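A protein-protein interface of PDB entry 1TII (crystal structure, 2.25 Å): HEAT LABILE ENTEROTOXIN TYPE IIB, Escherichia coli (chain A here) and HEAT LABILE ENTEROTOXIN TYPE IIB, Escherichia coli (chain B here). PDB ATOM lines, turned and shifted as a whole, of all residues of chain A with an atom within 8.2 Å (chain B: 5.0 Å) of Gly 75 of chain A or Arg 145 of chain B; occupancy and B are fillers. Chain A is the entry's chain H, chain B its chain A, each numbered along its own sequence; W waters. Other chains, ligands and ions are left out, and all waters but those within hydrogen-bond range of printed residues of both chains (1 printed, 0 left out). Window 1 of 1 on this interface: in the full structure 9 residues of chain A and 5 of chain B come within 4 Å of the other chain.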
ATOM      1  N   VAL A  21      22.327   5.836  27.210  1.00  0.00           N
ATOM      2  CA  VAL A  21      21.212   6.087  26.307  1.00  0.00           C
ATOM      3  C   VAL A  21      19.888   5.565  26.879  1.00  0.00           C
ATOM      4  O   VAL A  21      19.837   4.480  27.494  1.00  0.00           O
ATOM      5  CB  VAL A  21      21.451   5.431  24.946  1.00  0.00           C
ATOM      6  CG1 VAL A  21      20.327   5.791  23.979  1.00  0.00           C
ATOM      7  CG2 VAL A  21      22.796   5.864  24.392  1.00  0.00           C
ATOM      8  N   GLU A  22      18.839   6.372  26.726  1.00  0.00           N
ATOM      9  CA  GLU A  22      17.488   6.012  27.169  1.00  0.00           C
ATOM     10  C   GLU A  22      16.669   5.653  25.927  1.00  0.00           C
ATOM     11  O   GLU A  22      16.365   6.505  25.094  1.00  0.00           O
ATOM     12  CB  GLU A  22      16.863   7.180  27.927  1.00  0.00           C
ATOM     13  CG  GLU A  22      15.375   7.039  28.259  1.00  0.00           C
ATOM     14  CD  GLU A  22      15.054   5.830  29.118  1.00  0.00           C
ATOM     15  OE1 GLU A  22      15.724   5.632  30.167  1.00  0.00           O
ATOM     16  OE2 GLU A  22      14.127   5.077  28.735  1.00  0.00           O
ATOM     17  N   LEU A  23      16.454   4.365  25.732  1.00  0.00           N
ATOM     18  CA  LEU A  23      15.694   3.878  24.597  1.00  0.00           C
ATOM     19  C   LEU A  23      14.199   3.965  24.914  1.00  0.00           C
ATOM     20  O   LEU A  23      13.772   3.611  26.002  1.00  0.00           O
ATOM     21  CB  LEU A  23      16.076   2.433  24.317  1.00  0.00           C
ATOM     22  CG  LEU A  23      17.551   2.197  24.028  1.00  0.00           C
ATOM     23  CD1 LEU A  23      17.804   0.713  23.821  1.00  0.00           C
ATOM     24  CD2 LEU A  23      17.929   2.986  22.775  1.00  0.00           C
ATOM     25  N   THR A  24      13.398   4.422  23.961  1.00  0.00           N
ATOM     26  CA  THR A  24      11.974   4.540  24.205  1.00  0.00           C
ATOM     27  C   THR A  24      11.085   3.946  23.117  1.00  0.00           C
ATOM     28  O   THR A  24       9.864   3.899  23.248  1.00  0.00           O
ATOM     29  CB  THR A  24      11.605   6.000  24.448  1.00  0.00           C
ATOM     30  OG1 THR A  24      12.036   6.781  23.336  1.00  0.00           O
ATOM     31  CG2 THR A  24      12.282   6.513  25.702  1.00  0.00           C
ATOM     32  N   LYS A  25      11.695   3.449  22.057  1.00  0.00           N
ATOM     33  CA  LYS A  25      10.938   2.851  20.986  1.00  0.00           C
ATOM     34  C   LYS A  25      11.683   1.641  20.485  1.00  0.00           C
ATOM     35  O   LYS A  25      12.897   1.669  20.376  1.00  0.00           O
ATOM     36  CB  LYS A  25      10.730   3.843  19.854  1.00  0.00           C
ATOM     37  CG  LYS A  25       9.886   5.031  20.233  1.00  0.00           C
ATOM     38  CD  LYS A  25       9.548   5.837  18.995  1.00  0.00           C
ATOM     39  CE  LYS A  25       8.588   6.964  19.298  1.00  0.00           C
ATOM     40  NZ  LYS A  25       9.092   7.774  20.433  1.00  0.00           N
ATOM     41  N   VAL A  40      15.089   3.412  19.300  1.00  0.00           N
ATOM     42  CA  VAL A  40      15.117   4.872  19.217  1.00  0.00           C
ATOM     43  C   VAL A  40      15.313   5.407  20.607  1.00  0.00           C
ATOM     44  O   VAL A  40      14.739   4.887  21.559  1.00  0.00           O
ATOM     45  CB  VAL A  40      13.810   5.460  18.603  1.00  0.00           C
ATOM     46  CG1 VAL A  40      13.901   6.962  18.523  1.00  0.00           C
ATOM     47  CG2 VAL A  40      13.545   4.882  17.199  1.00  0.00           C
ATOM     48  N   SER A  42      15.480   8.565  23.497  1.00  0.00           N
ATOM     49  CA  SER A  42      14.560   9.625  23.853  1.00  0.00           C
ATOM     50  C   SER A  42      14.843  10.909  23.053  1.00  0.00           C
ATOM     51  O   SER A  42      14.011  11.835  23.024  1.00  0.00           O
ATOM     52  CB  SER A  42      14.693   9.909  25.343  1.00  0.00           C
ATOM     53  OG  SER A  42      16.023  10.287  25.671  1.00  0.00           O
ATOM     54  N   ALA A  68      17.399  -4.789  24.421  1.00  0.00           N
ATOM     55  CA  ALA A  68      16.692  -3.647  23.875  1.00  0.00           C
ATOM     56  C   ALA A  68      15.253  -3.637  24.407  1.00  0.00           C
ATOM     57  O   ALA A  68      14.762  -2.605  24.844  1.00  0.00           O
ATOM     58  CB  ALA A  68      16.711  -3.705  22.359  1.00  0.00           C
ATOM     59  N   MET A  69      14.595  -4.789  24.397  1.00  0.00           N
ATOM     60  CA  MET A  69      13.225  -4.914  24.895  1.00  0.00           C
ATOM     61  C   MET A  69      13.183  -4.517  26.365  1.00  0.00           C
ATOM     62  O   MET A  69      12.378  -3.687  26.774  1.00  0.00           O
ATOM     63  CB  MET A  69      12.741  -6.364  24.726  1.00  0.00           C
ATOM     64  CG  MET A  69      11.358  -6.689  25.315  1.00  0.00           C
ATOM     65  SD  MET A  69       9.985  -5.852  24.494  1.00  0.00           S
ATOM     66  CE  MET A  69       9.772  -6.851  23.142  1.00  0.00           C
ATOM     67  N   ALA A  70      14.082  -5.083  27.154  1.00  0.00           N
ATOM     68  CA  ALA A  70      14.142  -4.790  28.573  1.00  0.00           C
ATOM     69  C   ALA A  70      14.389  -3.326  28.878  1.00  0.00           C
ATOM     70  O   ALA A  70      13.826  -2.792  29.820  1.00  0.00           O
ATOM     71  CB  ALA A  70      15.199  -5.634  29.229  1.00  0.00           C
ATOM     72  N   ALA A  71      15.255  -2.683  28.103  1.00  0.00           N
ATOM     73  CA  ALA A  71      15.563  -1.279  28.309  1.00  0.00           C
ATOM     74  C   ALA A  71      14.351  -0.385  28.012  1.00  0.00           C
ATOM     75  O   ALA A  71      14.018   0.499  28.798  1.00  0.00           O
ATOM     76  CB  ALA A  71      16.750  -0.882  27.437  1.00  0.00           C
ATOM     77  N   VAL A  72      13.688  -0.620  26.884  1.00  0.00           N
ATOM     78  CA  VAL A  72      12.504   0.162  26.502  1.00  0.00           C
ATOM     79  C   VAL A  72      11.344   0.035  27.517  1.00  0.00           C
ATOM     80  O   VAL A  72      10.710   1.020  27.882  1.00  0.00           O
ATOM     81  CB  VAL A  72      12.004  -0.269  25.113  1.00  0.00           C
ATOM     82  CG1 VAL A  72      10.775   0.500  24.721  1.00  0.00           C
ATOM     83  CG2 VAL A  72      13.091  -0.046  24.095  1.00  0.00           C
ATOM     84  N   LEU A  73      11.081  -1.183  27.974  1.00  0.00           N
ATOM     85  CA  LEU A  73      10.007  -1.441  28.926  1.00  0.00           C
ATOM     86  C   LEU A  73      10.261  -0.834  30.277  1.00  0.00           C
ATOM     87  O   LEU A  73       9.401  -0.165  30.825  1.00  0.00           O
ATOM     88  CB  LEU A  73       9.811  -2.951  29.127  1.00  0.00           C
ATOM     89  CG  LEU A  73       9.044  -3.811  28.107  1.00  0.00           C
ATOM     90  CD1 LEU A  73       9.149  -5.262  28.528  1.00  0.00           C
ATOM     91  CD2 LEU A  73       7.569  -3.381  28.010  1.00  0.00           C
ATOM     92  N   SER A  74      11.437  -1.111  30.823  1.00  0.00           N
ATOM     93  CA  SER A  74      11.805  -0.669  32.157  1.00  0.00           C
ATOM     94  C   SER A  74      12.360   0.724  32.311  1.00  0.00           C
ATOM     95  O   SER A  74      12.368   1.241  33.411  1.00  0.00           O
ATOM     96  CB  SER A  74      12.835  -1.630  32.728  1.00  0.00           C
ATOM     97  OG  SER A  74      14.070  -1.501  32.022  1.00  0.00           O
ATOM     98  N   GLY A  75      12.952   1.261  31.253  1.00  0.00           N
ATOM     99  CA  GLY A  75      13.542   2.571  31.345  1.00  0.00           C
ATOM    100  C   GLY A  75      14.998   2.513  31.793  1.00  0.00           C
ATOM    101  O   GLY A  75      15.601   3.548  32.109  1.00  0.00           O
ATOM    102  N   MET A  76      15.566   1.313  31.878  1.00  0.00           N
ATOM    103  CA  MET A  76      16.983   1.184  32.252  1.00  0.00           C
ATOM    104  C   MET A  76      17.871   1.627  31.098  1.00  0.00           C
ATOM    105  O   MET A  76      17.573   1.367  29.936  1.00  0.00           O
ATOM    106  CB  MET A  76      17.331  -0.243  32.620  1.00  0.00           C
ATOM    107  CG  MET A  76      16.740  -0.661  33.918  1.00  0.00           C
ATOM    108  SD  MET A  76      16.992  -2.393  34.154  1.00  0.00           S
ATOM    109  CE  MET A  76      18.558  -2.430  34.854  1.00  0.00           C
ATOM    110  N   ARG A  77      18.983   2.265  31.409  1.00  0.00           N
ATOM    111  CA  ARG A  77      19.837   2.742  30.343  1.00  0.00           C
ATOM    112  C   ARG A  77      20.771   1.702  29.787  1.00  0.00           C
ATOM    113  O   ARG A  77      21.015   0.643  30.392  1.00  0.00           O
ATOM    114  CB  ARG A  77      20.615   3.952  30.804  1.00  0.00           C
ATOM    115  CG  ARG A  77      19.714   4.963  31.387  1.00  0.00           C
ATOM    116  CD  ARG A  77      20.419   6.196  31.735  1.00  0.00           C
ATOM    117  NE  ARG A  77      19.446   7.271  31.782  1.00  0.00           N
ATOM    118  CZ  ARG A  77      19.700   8.484  32.256  1.00  0.00           C
ATOM    119  NH1 ARG A  77      20.916   8.762  32.717  1.00  0.00           N
ATOM    120  NH2 ARG A  77      18.734   9.404  32.287  1.00  0.00           N
ATOM    121  N   VAL A  78      21.287   2.038  28.615  1.00  0.00           N
ATOM    122  CA  VAL A  78      22.225   1.203  27.893  1.00  0.00           C
ATOM    123  C   VAL A  78      23.428   2.032  27.383  1.00  0.00           C
ATOM    124  O   VAL A  78      23.353   3.253  27.244  1.00  0.00           O
ATOM    125  CB  VAL A  78      21.523   0.518  26.687  1.00  0.00           C
ATOM    126  CG1 VAL A  78      20.397  -0.411  27.177  1.00  0.00           C
ATOM    127  CG2 VAL A  78      20.957   1.568  25.762  1.00  0.00           C
ATOM    128  N   LEU A  96      23.665  -3.490  29.196  1.00  0.00           N
ATOM    129  CA  LEU A  96      22.499  -3.085  29.974  1.00  0.00           C
ATOM    130  C   LEU A  96      23.015  -2.705  31.343  1.00  0.00           C
ATOM    131  O   LEU A  96      23.729  -3.487  31.966  1.00  0.00           O
ATOM    132  CB  LEU A  96      21.502  -4.239  30.116  1.00  0.00           C
ATOM    133  CG  LEU A  96      20.231  -4.048  30.977  1.00  0.00           C
ATOM    134  CD1 LEU A  96      19.298  -3.055  30.318  1.00  0.00           C
ATOM    135  CD2 LEU A  96      19.519  -5.393  31.169  1.00  0.00           C
ATOM    136  N   GLU A  97      22.674  -1.512  31.816  1.00  0.00           N
ATOM    137  CA  GLU A  97      23.129  -1.093  33.132  1.00  0.00           C
ATOM    138  C   GLU A  97      21.982  -0.806  34.096  1.00  0.00           C
ATOM    139  O   GLU A  97      20.944  -0.296  33.694  1.00  0.00           O
ATOM    140  CB  GLU A  97      24.070   0.124  33.030  1.00  0.00           C
ATOM    141  CG  GLU A  97      23.510   1.388  32.372  1.00  0.00           C
ATOM    142  CD  GLU A  97      24.409   2.628  32.560  1.00  0.00           C
ATOM    143  OE1 GLU A  97      25.453   2.551  33.246  1.00  0.00           O
ATOM    144  OE2 GLU A  97      24.062   3.701  32.028  1.00  0.00           O
ATOM    145  N   TYR B 143      12.646   3.943  38.747  1.00  0.00           N
ATOM    146  CA  TYR B 143      11.242   4.033  38.415  1.00  0.00           C
ATOM    147  C   TYR B 143      11.005   2.975  37.347  1.00  0.00           C
ATOM    148  O   TYR B 143      11.812   2.845  36.438  1.00  0.00           O
ATOM    149  CB  TYR B 143      10.910   5.400  37.831  1.00  0.00           C
ATOM    150  CG  TYR B 143       9.478   5.499  37.367  1.00  0.00           C
ATOM    151  CD1 TYR B 143       8.430   5.140  38.207  1.00  0.00           C
ATOM    152  CD2 TYR B 143       9.172   5.907  36.079  1.00  0.00           C
ATOM    153  CE1 TYR B 143       7.123   5.183  37.778  1.00  0.00           C
ATOM    154  CE2 TYR B 143       7.870   5.953  35.643  1.00  0.00           C
ATOM    155  CZ  TYR B 143       6.851   5.585  36.502  1.00  0.00           C
ATOM    156  OH  TYR B 143       5.554   5.620  36.067  1.00  0.00           O
ATOM    157  N   ARG B 144       9.943   2.183  37.493  1.00  0.00           N
ATOM    158  CA  ARG B 144       9.605   1.138  36.527  1.00  0.00           C
ATOM    159  C   ARG B 144       8.303   1.500  35.813  1.00  0.00           C
ATOM    160  O   ARG B 144       7.224   1.148  36.264  1.00  0.00           O
ATOM    161  CB  ARG B 144       9.458  -0.214  37.222  1.00  0.00           C
ATOM    162  CG  ARG B 144      10.696  -0.743  37.930  1.00  0.00           C
ATOM    163  CD  ARG B 144      11.748  -1.335  36.981  1.00  0.00           C
ATOM    164  NE  ARG B 144      12.607  -0.288  36.429  1.00  0.00           N
ATOM    165  CZ  ARG B 144      13.890  -0.087  36.742  1.00  0.00           C
ATOM    166  NH1 ARG B 144      14.536  -0.875  37.606  1.00  0.00           N
ATOM    167  NH2 ARG B 144      14.488   0.998  36.262  1.00  0.00           N
ATOM    168  N   ARG B 145       8.414   2.198  34.693  1.00  0.00           N
ATOM    169  CA  ARG B 145       7.267   2.625  33.927  1.00  0.00           C
ATOM    170  C   ARG B 145       6.394   1.480  33.445  1.00  0.00           C
ATOM    171  O   ARG B 145       5.172   1.607  33.389  1.00  0.00           O
ATOM    172  CB  ARG B 145       7.707   3.470  32.734  1.00  0.00           C
ATOM    173  CG  ARG B 145       8.529   2.733  31.709  1.00  0.00           C
ATOM    174  CD  ARG B 145       8.896   3.687  30.612  1.00  0.00           C
ATOM    175  NE  ARG B 145       9.886   3.168  29.664  1.00  0.00           N
ATOM    176  CZ  ARG B 145      10.934   3.871  29.236  1.00  0.00           C
ATOM    177  NH1 ARG B 145      11.160   5.080  29.728  1.00  0.00           N
ATOM    178  NH2 ARG B 145      11.786   3.358  28.360  1.00  0.00           N
ATOM    179  N   ASP B 146       7.008   0.367  33.080  1.00  0.00           N
ATOM    180  CA  ASP B 146       6.238  -0.773  32.600  1.00  0.00           C
ATOM    181  C   ASP B 146       5.295  -1.343  33.670  1.00  0.00           C
ATOM    182  O   ASP B 146       4.348  -2.039  33.348  1.00  0.00           O
ATOM    183  CB  ASP B 146       7.173  -1.868  32.070  1.00  0.00           C
ATOM    184  CG  ASP B 146       8.160  -2.356  33.113  1.00  0.00           C
ATOM    185  OD1 ASP B 146       8.575  -1.563  33.980  1.00  0.00           O
ATOM    186  OD2 ASP B 146       8.538  -3.542  33.053  1.00  0.00           O
ATOM    187  N   LEU B 147       5.585  -1.079  34.934  1.00  0.00           N
ATOM    188  CA  LEU B 147       4.751  -1.577  36.017  1.00  0.00           C
ATOM    189  C   LEU B 147       3.606  -0.632  36.401  1.00  0.00           C
ATOM    190  O   LEU B 147       2.599  -1.062  36.989  1.00  0.00           O
ATOM    191  CB  LEU B 147       5.587  -1.830  37.276  1.00  0.00           C
ATOM    192  CG  LEU B 147       6.739  -2.827  37.335  1.00  0.00           C
ATOM    193  CD1 LEU B 147       7.092  -3.032  38.794  1.00  0.00           C
ATOM    194  CD2 LEU B 147       6.348  -4.156  36.690  1.00  0.00           C
ATOM    195  N   PHE B 148       3.776   0.654  36.109  1.00  0.00           N
ATOM    196  CA  PHE B 148       2.787   1.628  36.499  1.00  0.00           C
ATOM    197  C   PHE B 148       2.008   2.334  35.408  1.00  0.00           C
ATOM    198  O   PHE B 148       1.050   3.024  35.705  1.00  0.00           O
ATOM    199  CB  PHE B 148       3.422   2.612  37.469  1.00  0.00           C
ATOM    200  CG  PHE B 148       3.804   1.979  38.762  1.00  0.00           C
ATOM    201  CD1 PHE B 148       2.845   1.733  39.732  1.00  0.00           C
ATOM    202  CD2 PHE B 148       5.082   1.496  38.959  1.00  0.00           C
ATOM    203  CE1 PHE B 148       3.151   1.001  40.868  1.00  0.00           C
ATOM    204  CE2 PHE B 148       5.399   0.759  40.099  1.00  0.00           C
ATOM    205  CZ  PHE B 148       4.428   0.508  41.053  1.00  0.00           C
ATOM    206  N   ARG B 149       2.372   2.127  34.153  1.00  0.00           N
ATOM    207  CA  ARG B 149       1.685   2.760  33.040  1.00  0.00           C
ATOM    208  C   ARG B 149       0.185   2.436  33.050  1.00  0.00           C
ATOM    209  O   ARG B 149      -0.228   1.285  33.066  1.00  0.00           O
ATOM    210  CB  ARG B 149       2.324   2.292  31.725  1.00  0.00           C
ATOM    211  CG  ARG B 149       1.616   2.703  30.425  1.00  0.00           C
ATOM    212  CD  ARG B 149       1.642   4.207  30.187  1.00  0.00           C
ATOM    213  NE  ARG B 149       2.938   4.788  30.530  1.00  0.00           N
ATOM    214  CZ  ARG B 149       3.936   4.966  29.669  1.00  0.00           C
ATOM    215  NH1 ARG B 149       3.792   4.621  28.396  1.00  0.00           N
ATOM    216  NH2 ARG B 149       5.094   5.451  30.101  1.00  0.00           N
HETATM  217  O   HOH W   1      10.792   3.394  33.777  1.00  0.00           O
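Water W1 lies within hydrogen-bond range of the backbone carbonyl oxygen of Ser 74 of chain A (2.7 Å), the backbone NH of Arg 145 of chain B (2.8 Å) and the backbone carbonyl oxygen of Tyr 143 of chain B (2.9 Å).
Arg 145 of chain B touches Ala 71 of chain A (NH2 to O, 3.7 Å).
Arg 145 of chain B touches Leu 73 of chain A.
Asp 146 of chain B touches Ser 74 of chain A (OD1 to CA, 3.8 Å).
CA of Gly 75 of chain A touches NH2 of Arg 145 of chain B, at 3.6 Å.
Met 76 of chain A touches Arg 144 of chain B.
Val 40 of chain A touches none of the printed residues of chain B.
Printed residues of chain B within 4 Å of Leu 73 of chain A: Arg 145 (3.2 Å) and Asp 146 (3.1 Å).
Printed residues of chain B within 4 Å of Ser 74 of chain A: Tyr 143 (3.5 Å), Arg 144 (3.4 Å) and Asp 146 (3.8 Å).
Gly 75 of chain A touches one residue of chain B.
Leu 96 of chain A touches none of the printed residues of chain B.
Of the printed residues of chain A, Tyr 143 of chain B touches Ser 74 (3.5 Å).
Printed residues of chain A within 4 Å of Arg 145 of chain B: Glu 22 (2.9 Å), Leu 23 (3.1 Å), Ala 71 (3.7 Å), Val 72 (2.6 Å), Leu 73 (3.2 Å) and Gly 75 (3.6 Å).
The nearest residue of chain B that does not touch Gly 75 of chain A is Arg 144 of chain B (4.7 Å).
The nearest residue of chain A that does not touch Arg 145 of chain B is Thr 24 of chain A (4.2 Å).
The nearest printed residue of chain B that does not touch Leu 73 of chain A is Arg 144 of chain B (5.4 Å).
The guanidinium group (NH2) of Arg 145 of chain B is in salt-bridge range of the side-chain carboxylate (OE2) of Glu 22 of chain A (2.9 Å).
The guanidinium group (NH2) of Arg 145 of chain B lies within hydrogen-bond range of the backbone carbonyl oxygen (O) of Leu 23 of chain A, at 3.1 Å.
The guanidinium group (NH2) of Arg 145 of chain B is in hydrogen-bond range of the backbone carbonyl oxygen (O) of Val 72 of chain A (2.6 Å).
O of Leu 73 of chain A lies close to N of Asp 146 of chain B (3.3 Å).
O of Ser 74 of chain A is in hydrogen-bond range of NE of Arg 144 of chain B, 3.4 Å away.
O of Ser 74 of chain A lies close to O of Tyr 143 of chain B (3.5 Å).
Hydrophobic or aromatic side chains of chain A that line the printed part of chain B: Met 76.
The backbone carbonyl oxygen of Glu 22 of chain A sits at hydrogen-bond distance from the backbone NH of Ser 42 of chain A (2.8 Å).
OG of Ser 74 of chain A is in hydrogen-bond range of O of Ala 70 of chain A (2.6 Å).
The side-chain hydroxyl of Ser 74 of chain A sits at hydrogen-bond distance from the backbone NH of Met 76 of chain A (3.2 Å).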
